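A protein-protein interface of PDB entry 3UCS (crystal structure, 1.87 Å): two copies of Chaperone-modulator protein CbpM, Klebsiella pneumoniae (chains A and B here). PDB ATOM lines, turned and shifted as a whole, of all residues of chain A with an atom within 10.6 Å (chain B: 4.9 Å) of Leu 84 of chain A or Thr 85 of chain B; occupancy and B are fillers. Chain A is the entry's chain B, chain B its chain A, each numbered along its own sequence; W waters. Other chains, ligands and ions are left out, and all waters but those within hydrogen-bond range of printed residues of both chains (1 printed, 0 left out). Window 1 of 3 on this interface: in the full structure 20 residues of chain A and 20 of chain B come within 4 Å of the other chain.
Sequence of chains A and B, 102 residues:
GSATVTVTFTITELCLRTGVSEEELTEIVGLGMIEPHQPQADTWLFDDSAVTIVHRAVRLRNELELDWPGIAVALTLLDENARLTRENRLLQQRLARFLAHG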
ATOM      1  N   THR A  76       2.978  25.867   2.696  1.00  0.00           N
ATOM      2  CA  THR A  76       3.120  25.708   1.241  1.00  0.00           C
ATOM      3  C   THR A  76       4.329  24.826   0.885  1.00  0.00           C
ATOM      4  O   THR A  76       4.225  23.946   0.021  1.00  0.00           O
ATOM      5  CB  THR A  76       3.156  27.056   0.507  1.00  0.00           C
ATOM      6  OG1 THR A  76       1.875  27.695   0.645  1.00  0.00           O
ATOM      7  CG2 THR A  76       3.490  26.886  -1.000  1.00  0.00           C
ATOM      8  N   LEU A  77       5.455  25.056   1.556  1.00  0.00           N
ATOM      9  CA  LEU A  77       6.661  24.249   1.327  1.00  0.00           C
ATOM     10  C   LEU A  77       6.504  22.805   1.833  1.00  0.00           C
ATOM     11  O   LEU A  77       6.913  21.845   1.183  1.00  0.00           O
ATOM     12  CB  LEU A  77       7.868  24.937   1.982  1.00  0.00           C
ATOM     13  CG  LEU A  77       8.352  26.226   1.292  1.00  0.00           C
ATOM     14  CD1 LEU A  77       9.346  26.917   2.230  1.00  0.00           C
ATOM     15  CD2 LEU A  77       9.019  25.892  -0.028  1.00  0.00           C
ATOM     16  N   LEU A  78       5.937  22.640   3.018  1.00  0.00           N
ATOM     17  CA  LEU A  78       5.637  21.286   3.493  1.00  0.00           C
ATOM     18  C   LEU A  78       4.777  20.494   2.502  1.00  0.00           C
ATOM     19  O   LEU A  78       5.056  19.328   2.230  1.00  0.00           O
ATOM     20  CB  LEU A  78       4.928  21.361   4.843  1.00  0.00           C
ATOM     21  CG  LEU A  78       5.852  21.745   5.994  1.00  0.00           C
ATOM     22  CD1 LEU A  78       4.998  22.084   7.210  1.00  0.00           C
ATOM     23  CD2 LEU A  78       6.851  20.600   6.315  1.00  0.00           C
ATOM     24  N   ASP A  79       3.758  21.136   1.944  1.00  0.00           N
ATOM     25  CA  ASP A  79       2.850  20.454   1.010  1.00  0.00           C
ATOM     26  C   ASP A  79       3.512  20.148  -0.326  1.00  0.00           C
ATOM     27  O   ASP A  79       3.292  19.074  -0.905  1.00  0.00           O
ATOM     28  CB  ASP A  79       1.553  21.247   0.818  1.00  0.00           C
ATOM     29  CG  ASP A  79       0.663  21.239   2.082  1.00  0.00           C
ATOM     30  OD1 ASP A  79       0.832  20.357   2.947  1.00  0.00           O
ATOM     31  OD2 ASP A  79      -0.189  22.129   2.230  1.00  0.00           O
ATOM     32  N   GLU A  80       4.339  21.074  -0.799  1.00  0.00           N
ATOM     33  CA  GLU A  80       5.113  20.825  -2.013  1.00  0.00           C
ATOM     34  C   GLU A  80       6.125  19.687  -1.808  1.00  0.00           C
ATOM     35  O   GLU A  80       6.247  18.808  -2.670  1.00  0.00           O
ATOM     36  CB  GLU A  80       5.788  22.113  -2.498  1.00  0.00           C
ATOM     37  CG  GLU A  80       6.718  21.979  -3.732  1.00  0.00           C
ATOM     38  CD  GLU A  80       6.049  21.348  -4.963  1.00  0.00           C
ATOM     39  OE1 GLU A  80       4.808  21.283  -5.028  1.00  0.00           O
ATOM     40  OE2 GLU A  80       6.774  20.901  -5.881  1.00  0.00           O
ATOM     41  N   ASN A  81       6.837  19.703  -0.683  1.00  0.00           N
ATOM     42  CA  ASN A  81       7.769  18.606  -0.370  1.00  0.00           C
ATOM     43  C   ASN A  81       7.066  17.264  -0.242  1.00  0.00           C
ATOM     44  O   ASN A  81       7.564  16.246  -0.733  1.00  0.00           O
ATOM     45  CB  ASN A  81       8.606  18.914   0.870  1.00  0.00           C
ATOM     46  CG  ASN A  81       9.592  20.072   0.616  1.00  0.00           C
ATOM     47  OD1 ASN A  81       9.771  20.478  -0.522  1.00  0.00           O
ATOM     48  ND2 ASN A  81      10.200  20.603   1.666  1.00  0.00           N
ATOM     49  N   ALA A  82       5.902  17.279   0.403  1.00  0.00           N
ATOM     50  CA  ALA A  82       5.111  16.053   0.532  1.00  0.00           C
ATOM     51  C   ALA A  82       4.690  15.574  -0.860  1.00  0.00           C
ATOM     52  O   ALA A  82       4.756  14.376  -1.138  1.00  0.00           O
ATOM     53  CB  ALA A  82       3.906  16.267   1.424  1.00  0.00           C
ATOM     54  N   ARG A  83       4.303  16.500  -1.733  1.00  0.00           N
ATOM     55  CA  ARG A  83       3.919  16.151  -3.107  1.00  0.00           C
ATOM     56  C   ARG A  83       5.091  15.537  -3.863  1.00  0.00           C
ATOM     57  O   ARG A  83       4.924  14.534  -4.538  1.00  0.00           O
ATOM     58  CB  ARG A  83       3.382  17.364  -3.886  1.00  0.00           C
ATOM     59  CG  ARG A  83       2.809  17.014  -5.253  1.00  0.00           C
ATOM     60  CD  ARG A  83       2.718  18.238  -6.169  1.00  0.00           C
ATOM     61  NE  ARG A  83       4.047  18.787  -6.473  1.00  0.00           N
ATOM     62  CZ  ARG A  83       4.906  18.259  -7.341  1.00  0.00           C
ATOM     63  NH1 ARG A  83       4.587  17.161  -8.012  1.00  0.00           N
ATOM     64  NH2 ARG A  83       6.090  18.833  -7.545  1.00  0.00           N
ATOM     65  N   LEU A  84       6.265  16.151  -3.752  1.00  0.00           N
ATOM     66  CA  LEU A  84       7.470  15.615  -4.398  1.00  0.00           C
ATOM     67  C   LEU A  84       7.868  14.257  -3.834  1.00  0.00           C
ATOM     68  O   LEU A  84       8.313  13.371  -4.559  1.00  0.00           O
ATOM     69  CB  LEU A  84       8.643  16.586  -4.214  1.00  0.00           C
ATOM     70  CG  LEU A  84       8.794  17.778  -5.149  1.00  0.00           C
ATOM     71  CD1 LEU A  84       9.925  18.679  -4.616  1.00  0.00           C
ATOM     72  CD2 LEU A  84       9.130  17.331  -6.579  1.00  0.00           C
ATOM     73  N   THR A  85       7.748  14.097  -2.528  1.00  0.00           N
ATOM     74  CA  THR A  85       8.019  12.808  -1.902  1.00  0.00           C
ATOM     75  C   THR A  85       7.122  11.719  -2.507  1.00  0.00           C
ATOM     76  O   THR A  85       7.605  10.625  -2.857  1.00  0.00           O
ATOM     77  CB  THR A  85       7.814  12.906  -0.385  1.00  0.00           C
ATOM     78  OG1 THR A  85       8.805  13.789   0.170  1.00  0.00           O
ATOM     79  CG2 THR A  85       7.898  11.517   0.296  1.00  0.00           C
ATOM     80  N   ARG A  86       5.831  12.011  -2.633  1.00  0.00           N
ATOM     81  CA  ARG A  86       4.908  11.066  -3.276  1.00  0.00           C
ATOM     82  C   ARG A  86       5.318  10.781  -4.718  1.00  0.00           C
ATOM     83  O   ARG A  86       5.332   9.613  -5.104  1.00  0.00           O
ATOM     84  CB  ARG A  86       3.443  11.528  -3.184  1.00  0.00           C
ATOM     85  CG  ARG A  86       2.868  11.482  -1.757  1.00  0.00           C
ATOM     86  CD  ARG A  86       1.366  11.872  -1.696  1.00  0.00           C
ATOM     87  NE  ARG A  86       1.036  13.154  -2.346  1.00  0.00           N
ATOM     88  CZ  ARG A  86       0.989  14.356  -1.748  1.00  0.00           C
ATOM     89  NH1 ARG A  86       1.279  14.507  -0.461  1.00  0.00           N
ATOM     90  NH2 ARG A  86       0.648  15.428  -2.457  1.00  0.00           N
ATOM     91  N   GLU A  87       5.666  11.828  -5.490  1.00  0.00           N
ATOM     92  CA  GLU A  87       6.120  11.641  -6.873  1.00  0.00           C
ATOM     93  C   GLU A  87       7.365  10.761  -6.932  1.00  0.00           C
ATOM     94  O   GLU A  87       7.428   9.849  -7.763  1.00  0.00           O
ATOM     95  CB  GLU A  87       6.372  12.968  -7.613  1.00  0.00           C
ATOM     96  CG  GLU A  87       6.983  12.742  -9.007  1.00  0.00           C
ATOM     97  CD  GLU A  87       7.170  14.001  -9.840  1.00  0.00           C
ATOM     98  OE1 GLU A  87       6.519  15.031  -9.546  1.00  0.00           O
ATOM     99  OE2 GLU A  87       7.966  13.941 -10.811  1.00  0.00           O
ATOM    100  N   ASN A  88       8.345  11.033  -6.059  1.00  0.00           N
ATOM    101  CA  ASN A  88       9.570  10.212  -6.009  1.00  0.00           C
ATOM    102  C   ASN A  88       9.291   8.743  -5.705  1.00  0.00           C
ATOM    103  O   ASN A  88       9.854   7.865  -6.349  1.00  0.00           O
ATOM    104  CB  ASN A  88      10.608  10.786  -5.041  1.00  0.00           C
ATOM    105  CG  ASN A  88      11.167  12.119  -5.535  1.00  0.00           C
ATOM    106  OD1 ASN A  88      10.832  12.554  -6.624  1.00  0.00           O
ATOM    107  ND2 ASN A  88      12.012  12.759  -4.732  1.00  0.00           N
ATOM    108  N   ARG A  89       8.414   8.479  -4.738  1.00  0.00           N
ATOM    109  CA  ARG A  89       7.995   7.097  -4.460  1.00  0.00           C
ATOM    110  C   ARG A  89       7.369   6.427  -5.687  1.00  0.00           C
ATOM    111  O   ARG A  89       7.643   5.239  -5.964  1.00  0.00           O
ATOM    112  CB  ARG A  89       7.028   7.044  -3.268  1.00  0.00           C
ATOM    113  CG  ARG A  89       6.467   5.646  -2.961  1.00  0.00           C
ATOM    114  CD  ARG A  89       5.987   5.490  -1.504  1.00  0.00           C
ATOM    115  NE  ARG A  89       4.762   6.241  -1.225  1.00  0.00           N
ATOM    116  CZ  ARG A  89       4.723   7.466  -0.693  1.00  0.00           C
ATOM    117  NH1 ARG A  89       5.846   8.101  -0.364  1.00  0.00           N
ATOM    118  NH2 ARG A  89       3.549   8.059  -0.482  1.00  0.00           N
ATOM    119  N   LEU A  90       6.538   7.178  -6.411  1.00  0.00           N
ATOM    120  CA  LEU A  90       5.936   6.671  -7.636  1.00  0.00           C
ATOM    121  C   LEU A  90       6.995   6.320  -8.678  1.00  0.00           C
ATOM    122  O   LEU A  90       6.899   5.287  -9.351  1.00  0.00           O
ATOM    123  CB  LEU A  90       4.939   7.673  -8.227  1.00  0.00           C
ATOM    124  CG  LEU A  90       4.179   7.311  -9.496  1.00  0.00           C
ATOM    125  CD1 LEU A  90       3.410   5.980  -9.322  1.00  0.00           C
ATOM    126  CD2 LEU A  90       3.235   8.444  -9.902  1.00  0.00           C
ATOM    127  N   LEU A  91       7.984   7.197  -8.844  1.00  0.00           N
ATOM    128  CA  LEU A  91       9.008   6.932  -9.841  1.00  0.00           C
ATOM    129  C   LEU A  91       9.816   5.718  -9.431  1.00  0.00           C
ATOM    130  O   LEU A  91      10.193   4.941 -10.287  1.00  0.00           O
ATOM    131  CB  LEU A  91       9.942   8.129 -10.034  1.00  0.00           C
ATOM    132  CG  LEU A  91       9.332   9.424 -10.575  1.00  0.00           C
ATOM    133  CD1 LEU A  91      10.465  10.481 -10.684  1.00  0.00           C
ATOM    134  CD2 LEU A  91       8.668   9.178 -11.944  1.00  0.00           C
ATOM    135  N   GLN A  92      10.088   5.564  -8.130  1.00  0.00           N
ATOM    136  CA  GLN A  92      10.806   4.388  -7.632  1.00  0.00           C
ATOM    137  C   GLN A  92      10.013   3.120  -7.932  1.00  0.00           C
ATOM    138  O   GLN A  92      10.586   2.115  -8.339  1.00  0.00           O
ATOM    139  CB  GLN A  92      11.069   4.490  -6.120  1.00  0.00           C
ATOM    140  CG  GLN A  92      12.192   3.579  -5.610  1.00  0.00           C
ATOM    141  CD  GLN A  92      13.592   4.146  -5.887  1.00  0.00           C
ATOM    142  OE1 GLN A  92      14.069   5.043  -5.175  1.00  0.00           O
ATOM    143  NE2 GLN A  92      14.263   3.603  -6.901  1.00  0.00           N
ATOM    144  N   ASN B  81      13.439  20.780  -0.135  1.00  0.00           N
ATOM    145  CA  ASN B  81      12.899  20.804  -1.493  1.00  0.00           C
ATOM    146  C   ASN B  81      13.994  20.513  -2.550  1.00  0.00           C
ATOM    147  O   ASN B  81      13.772  19.748  -3.501  1.00  0.00           O
ATOM    148  CB  ASN B  81      12.230  22.156  -1.775  1.00  0.00           C
ATOM    149  CG  ASN B  81      11.625  22.227  -3.143  1.00  0.00           C
ATOM    150  OD1 ASN B  81      12.257  22.691  -4.088  1.00  0.00           O
ATOM    151  ND2 ASN B  81      10.397  21.731  -3.275  1.00  0.00           N
ATOM    152  N   ALA B  82      15.161  21.144  -2.385  1.00  0.00           N
ATOM    153  CA  ALA B  82      16.255  20.966  -3.348  1.00  0.00           C
ATOM    154  C   ALA B  82      16.754  19.502  -3.295  1.00  0.00           C
ATOM    155  O   ALA B  82      17.006  18.881  -4.348  1.00  0.00           O
ATOM    156  CB  ALA B  82      17.413  21.987  -3.080  1.00  0.00           C
ATOM    157  N   ARG B  83      16.831  18.934  -2.087  1.00  0.00           N
ATOM    158  CA  ARG B  83      17.229  17.538  -1.952  1.00  0.00           C
ATOM    159  C   ARG B  83      16.252  16.614  -2.690  1.00  0.00           C
ATOM    160  O   ARG B  83      16.675  15.712  -3.414  1.00  0.00           O
ATOM    161  CB  ARG B  83      17.320  17.129  -0.481  1.00  0.00           C
ATOM    162  CG  ARG B  83      17.819  15.692  -0.256  1.00  0.00           C
ATOM    163  CD  ARG B  83      17.631  15.243   1.210  1.00  0.00           C
ATOM    164  NE  ARG B  83      16.239  14.954   1.568  1.00  0.00           N
ATOM    165  CZ  ARG B  83      15.590  13.833   1.229  1.00  0.00           C
ATOM    166  NH1 ARG B  83      16.193  12.903   0.485  1.00  0.00           N
ATOM    167  NH2 ARG B  83      14.333  13.648   1.607  1.00  0.00           N
ATOM    168  N   LEU B  84      14.955  16.834  -2.490  1.00  0.00           N
ATOM    169  CA  LEU B  84      13.936  15.994  -3.122  1.00  0.00           C
ATOM    170  C   LEU B  84      13.942  16.168  -4.636  1.00  0.00           C
ATOM    171  O   LEU B  84      13.720  15.225  -5.390  1.00  0.00           O
ATOM    172  CB  LEU B  84      12.560  16.321  -2.533  1.00  0.00           C
ATOM    173  CG  LEU B  84      12.323  15.817  -1.108  1.00  0.00           C
ATOM    174  CD1 LEU B  84      11.070  16.500  -0.492  1.00  0.00           C
ATOM    175  CD2 LEU B  84      12.156  14.288  -1.090  1.00  0.00           C
ATOM    176  N   THR B  85      14.189  17.399  -5.082  1.00  0.00           N
ATOM    177  CA  THR B  85      14.308  17.687  -6.504  1.00  0.00           C
ATOM    178  C   THR B  85      15.511  16.971  -7.160  1.00  0.00           C
ATOM    179  O   THR B  85      15.371  16.421  -8.268  1.00  0.00           O
ATOM    180  CB  THR B  85      14.330  19.204  -6.756  1.00  0.00           C
ATOM    181  OG1 THR B  85      13.114  19.763  -6.256  1.00  0.00           O
ATOM    182  CG2 THR B  85      14.427  19.509  -8.235  1.00  0.00           C
ATOM    183  N   ARG B  86      16.672  16.978  -6.496  1.00  0.00           N
ATOM    184  CA  ARG B  86      17.858  16.241  -6.987  1.00  0.00           C
ATOM    185  C   ARG B  86      17.550  14.747  -7.093  1.00  0.00           C
ATOM    186  O   ARG B  86      17.909  14.080  -8.085  1.00  0.00           O
ATOM    187  CB  ARG B  86      19.091  16.451  -6.090  1.00  0.00           C
ATOM    188  CG  ARG B  86      19.740  17.834  -6.197  1.00  0.00           C
ATOM    189  CD  ARG B  86      21.050  17.932  -5.398  1.00  0.00           C
ATOM    190  NE  ARG B  86      20.910  17.692  -3.949  1.00  0.00           N
ATOM    191  CZ  ARG B  86      20.595  18.629  -3.051  1.00  0.00           C
ATOM    192  NH1 ARG B  86      20.359  19.889  -3.428  1.00  0.00           N
ATOM    193  NH2 ARG B  86      20.552  18.315  -1.771  1.00  0.00           N
ATOM    194  N   GLU B  87      16.880  14.219  -6.075  1.00  0.00           N
ATOM    195  CA  GLU B  87      16.447  12.813  -6.097  1.00  0.00           C
ATOM    196  C   GLU B  87      15.445  12.520  -7.242  1.00  0.00           C
ATOM    197  O   GLU B  87      15.579  11.506  -7.940  1.00  0.00           O
ATOM    198  CB  GLU B  87      15.894  12.424  -4.720  1.00  0.00           C
ATOM    199  CG  GLU B  87      15.345  10.993  -4.612  1.00  0.00           C
ATOM    200  CD  GLU B  87      14.622  10.752  -3.301  1.00  0.00           C
ATOM    201  OE1 GLU B  87      15.164   9.999  -2.473  1.00  0.00           O
ATOM    202  OE2 GLU B  87      13.517  11.327  -3.085  1.00  0.00           O
ATOM    203  N   ASN B  88      14.469  13.408  -7.441  1.00  0.00           N
ATOM    204  CA  ASN B  88      13.501  13.294  -8.520  1.00  0.00           C
ATOM    205  C   ASN B  88      14.213  13.212  -9.856  1.00  0.00           C
ATOM    206  O   ASN B  88      13.911  12.358 -10.689  1.00  0.00           O
ATOM    207  CB  ASN B  88      12.546  14.505  -8.531  1.00  0.00           C
ATOM    208  CG  ASN B  88      11.479  14.402  -9.614  1.00  0.00           C
ATOM    209  OD1 ASN B  88      11.641  14.931 -10.710  1.00  0.00           O
ATOM    210  ND2 ASN B  88      10.375  13.718  -9.305  1.00  0.00           N
ATOM    211  N   ARG B  89      15.182  14.096 -10.054  1.00  0.00           N
ATOM    212  CA  ARG B  89      15.912  14.127 -11.315  1.00  0.00           C
ATOM    213  C   ARG B  89      16.724  12.873 -11.545  1.00  0.00           C
ATOM    214  O   ARG B  89      16.785  12.376 -12.673  1.00  0.00           O
ATOM    215  CB  ARG B  89      16.849  15.333 -11.370  1.00  0.00           C
ATOM    216  CG  ARG B  89      16.338  16.411 -12.250  1.00  0.00           C
ATOM    217  CD  ARG B  89      15.618  17.461 -11.447  1.00  0.00           C
ATOM    218  NE  ARG B  89      14.227  17.141 -11.117  1.00  0.00           N
ATOM    219  CZ  ARG B  89      13.190  17.878 -11.505  1.00  0.00           C
ATOM    220  NH1 ARG B  89      13.384  18.964 -12.248  1.00  0.00           N
ATOM    221  NH2 ARG B  89      11.960  17.542 -11.147  1.00  0.00           N
HETATM  222  O   HOH W   1       9.319  21.905  -5.879  1.00  0.00           O
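The side-chain amide oxygen (OD1) of Asn 81 of chain A is in hydrogen-bond range of the side-chain amide nitrogen (ND2) of Asn 81 of chain B, at 3.1 Å.
The backbone carbonyl oxygen (O) of Leu 84 of chain B is in hydrogen-bond range of the side-chain amide nitrogen (ND2) of Asn 88 of chain A (3.1 Å).
OE2 of Glu 87 of chain B lies within hydrogen-bond range of ND2 of Asn 88 of chain A (2.7 Å).
The side-chain amide nitrogen of Asn 88 of chain B is in hydrogen-bond range of the side-chain carboxylate of Glu 87 of chain A, 2.8 Å away.
The side-chain amide nitrogen (ND2) of Asn 88 of chain B lies within hydrogen-bond range of the side-chain amide oxygen (OD1) of Asn 88 of chain A, 3.0 Å away.
O of Asn 81 of chain B lies within hydrogen-bond range of OG1 of Thr 85 of chain B (2.8 Å).
The guanidinium group (NE) of Arg 89 of chain B sits at hydrogen-bond distance from the backbone carbonyl oxygen (O) of Thr 85 of chain B (3.2 Å).
OD1 of Asn 88 of chain B is in hydrogen-bond range of NH2 of Arg 89 of chain B, at 2.7 Å.
OE2 of Glu 80 of chain A lies within salt-bridge range of NH2 of Arg 83 of chain A, 2.7 Å away.
The side-chain carboxylate of Glu 87 of chain A lies within salt-bridge range of the guanidinium group of Arg 83 of chain A (3.3 Å).
O of Leu 84 of chain A lies close to OD1 of Asn 88 of chain A, 3.4 Å away.
Among the printed residues, pairs that only touch across the chains: Glu 80 of chain A with Asn 81 of chain B, Asn 81 of chain A with Leu 84 of chain B, Leu 84 of chain A with Asn 81 of chain B, Leu 84 of chain A with Thr 85 of chain B, Thr 85 of chain A with Leu 84 of chain B and Leu 91 of chain A with Asn 88 of chain B.
Leu 84 of chain A touches just these residues of chain B: Asn 81 and Thr 85.
Thr 85 of chain B touches just one residue of chain A: Leu 84.
Leu 84 of chain B touches just these residues of chain A: Asn 81 (3.5 Å), Thr 85 (3.6 Å) and Asn 88 (3.1 Å).
No residue of chain A comes within 4 Å of Arg 89 of chain B.
Of the printed residues of chain A, Asn 88 of chain B touches Glu 87 (2.8 Å), Asn 88 (3.0 Å) and Leu 91 (3.5 Å).
Of the printed residues of chain B, Glu 80 of chain A touches Asn 81 (3.7 Å).
Of the printed residues of chain B, Glu 87 of chain A touches Asn 88.
Of the printed residues of chain B, Thr 85 of chain A touches Leu 84 (3.6 Å).
Of the printed residues of chain A, Glu 87 of chain B touches Asn 88 (2.7 Å).
Arg 86 of chain B touches none of the printed residues of chain A.
The nearest residue of chain A that does not touch Thr 85 of chain B is Asn 88 of chain A (5.1 Å).
Of the 17 printed residues of chain A, 7 touch a printed residue of chain B.
Hydrophobic or aromatic side chains of chain B that line the printed part of chain A: Leu 84.
Among the printed residues, no Asp or Glu carboxylate lies within 4 Å of a Lys or Arg side-chain nitrogen of the other chain.
Asn 81 of chain A touches Leu 84 of chain B, and with the chains exchanged Leu 84 of chain A touches Asn 81 of chain B.
Leu 84 of chain A touches Thr 85 of chain B, and with the chains exchanged Thr 85 of chain A touches Leu 84 of chain B.
Asn 88 of chain A touches Leu 84 of chain B, but with the chains exchanged Leu 84 of chain A does not touch Asn 88 of chain B (4.7 Å).
Asn 88 of chain B touches its own counterpart, Asn 88 of chain A.
Of the 11 pairs that touch across the chains among the printed residues, 8 have their exchanged pair printed and touching as well.
Water W1 lies within hydrogen-bond range of the side-chain carboxylate (OE2) of Glu 80 of chain A (2.7 Å) and the side-chain amide nitrogen (ND2) of Asn 81 of chain B (2.8 Å).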
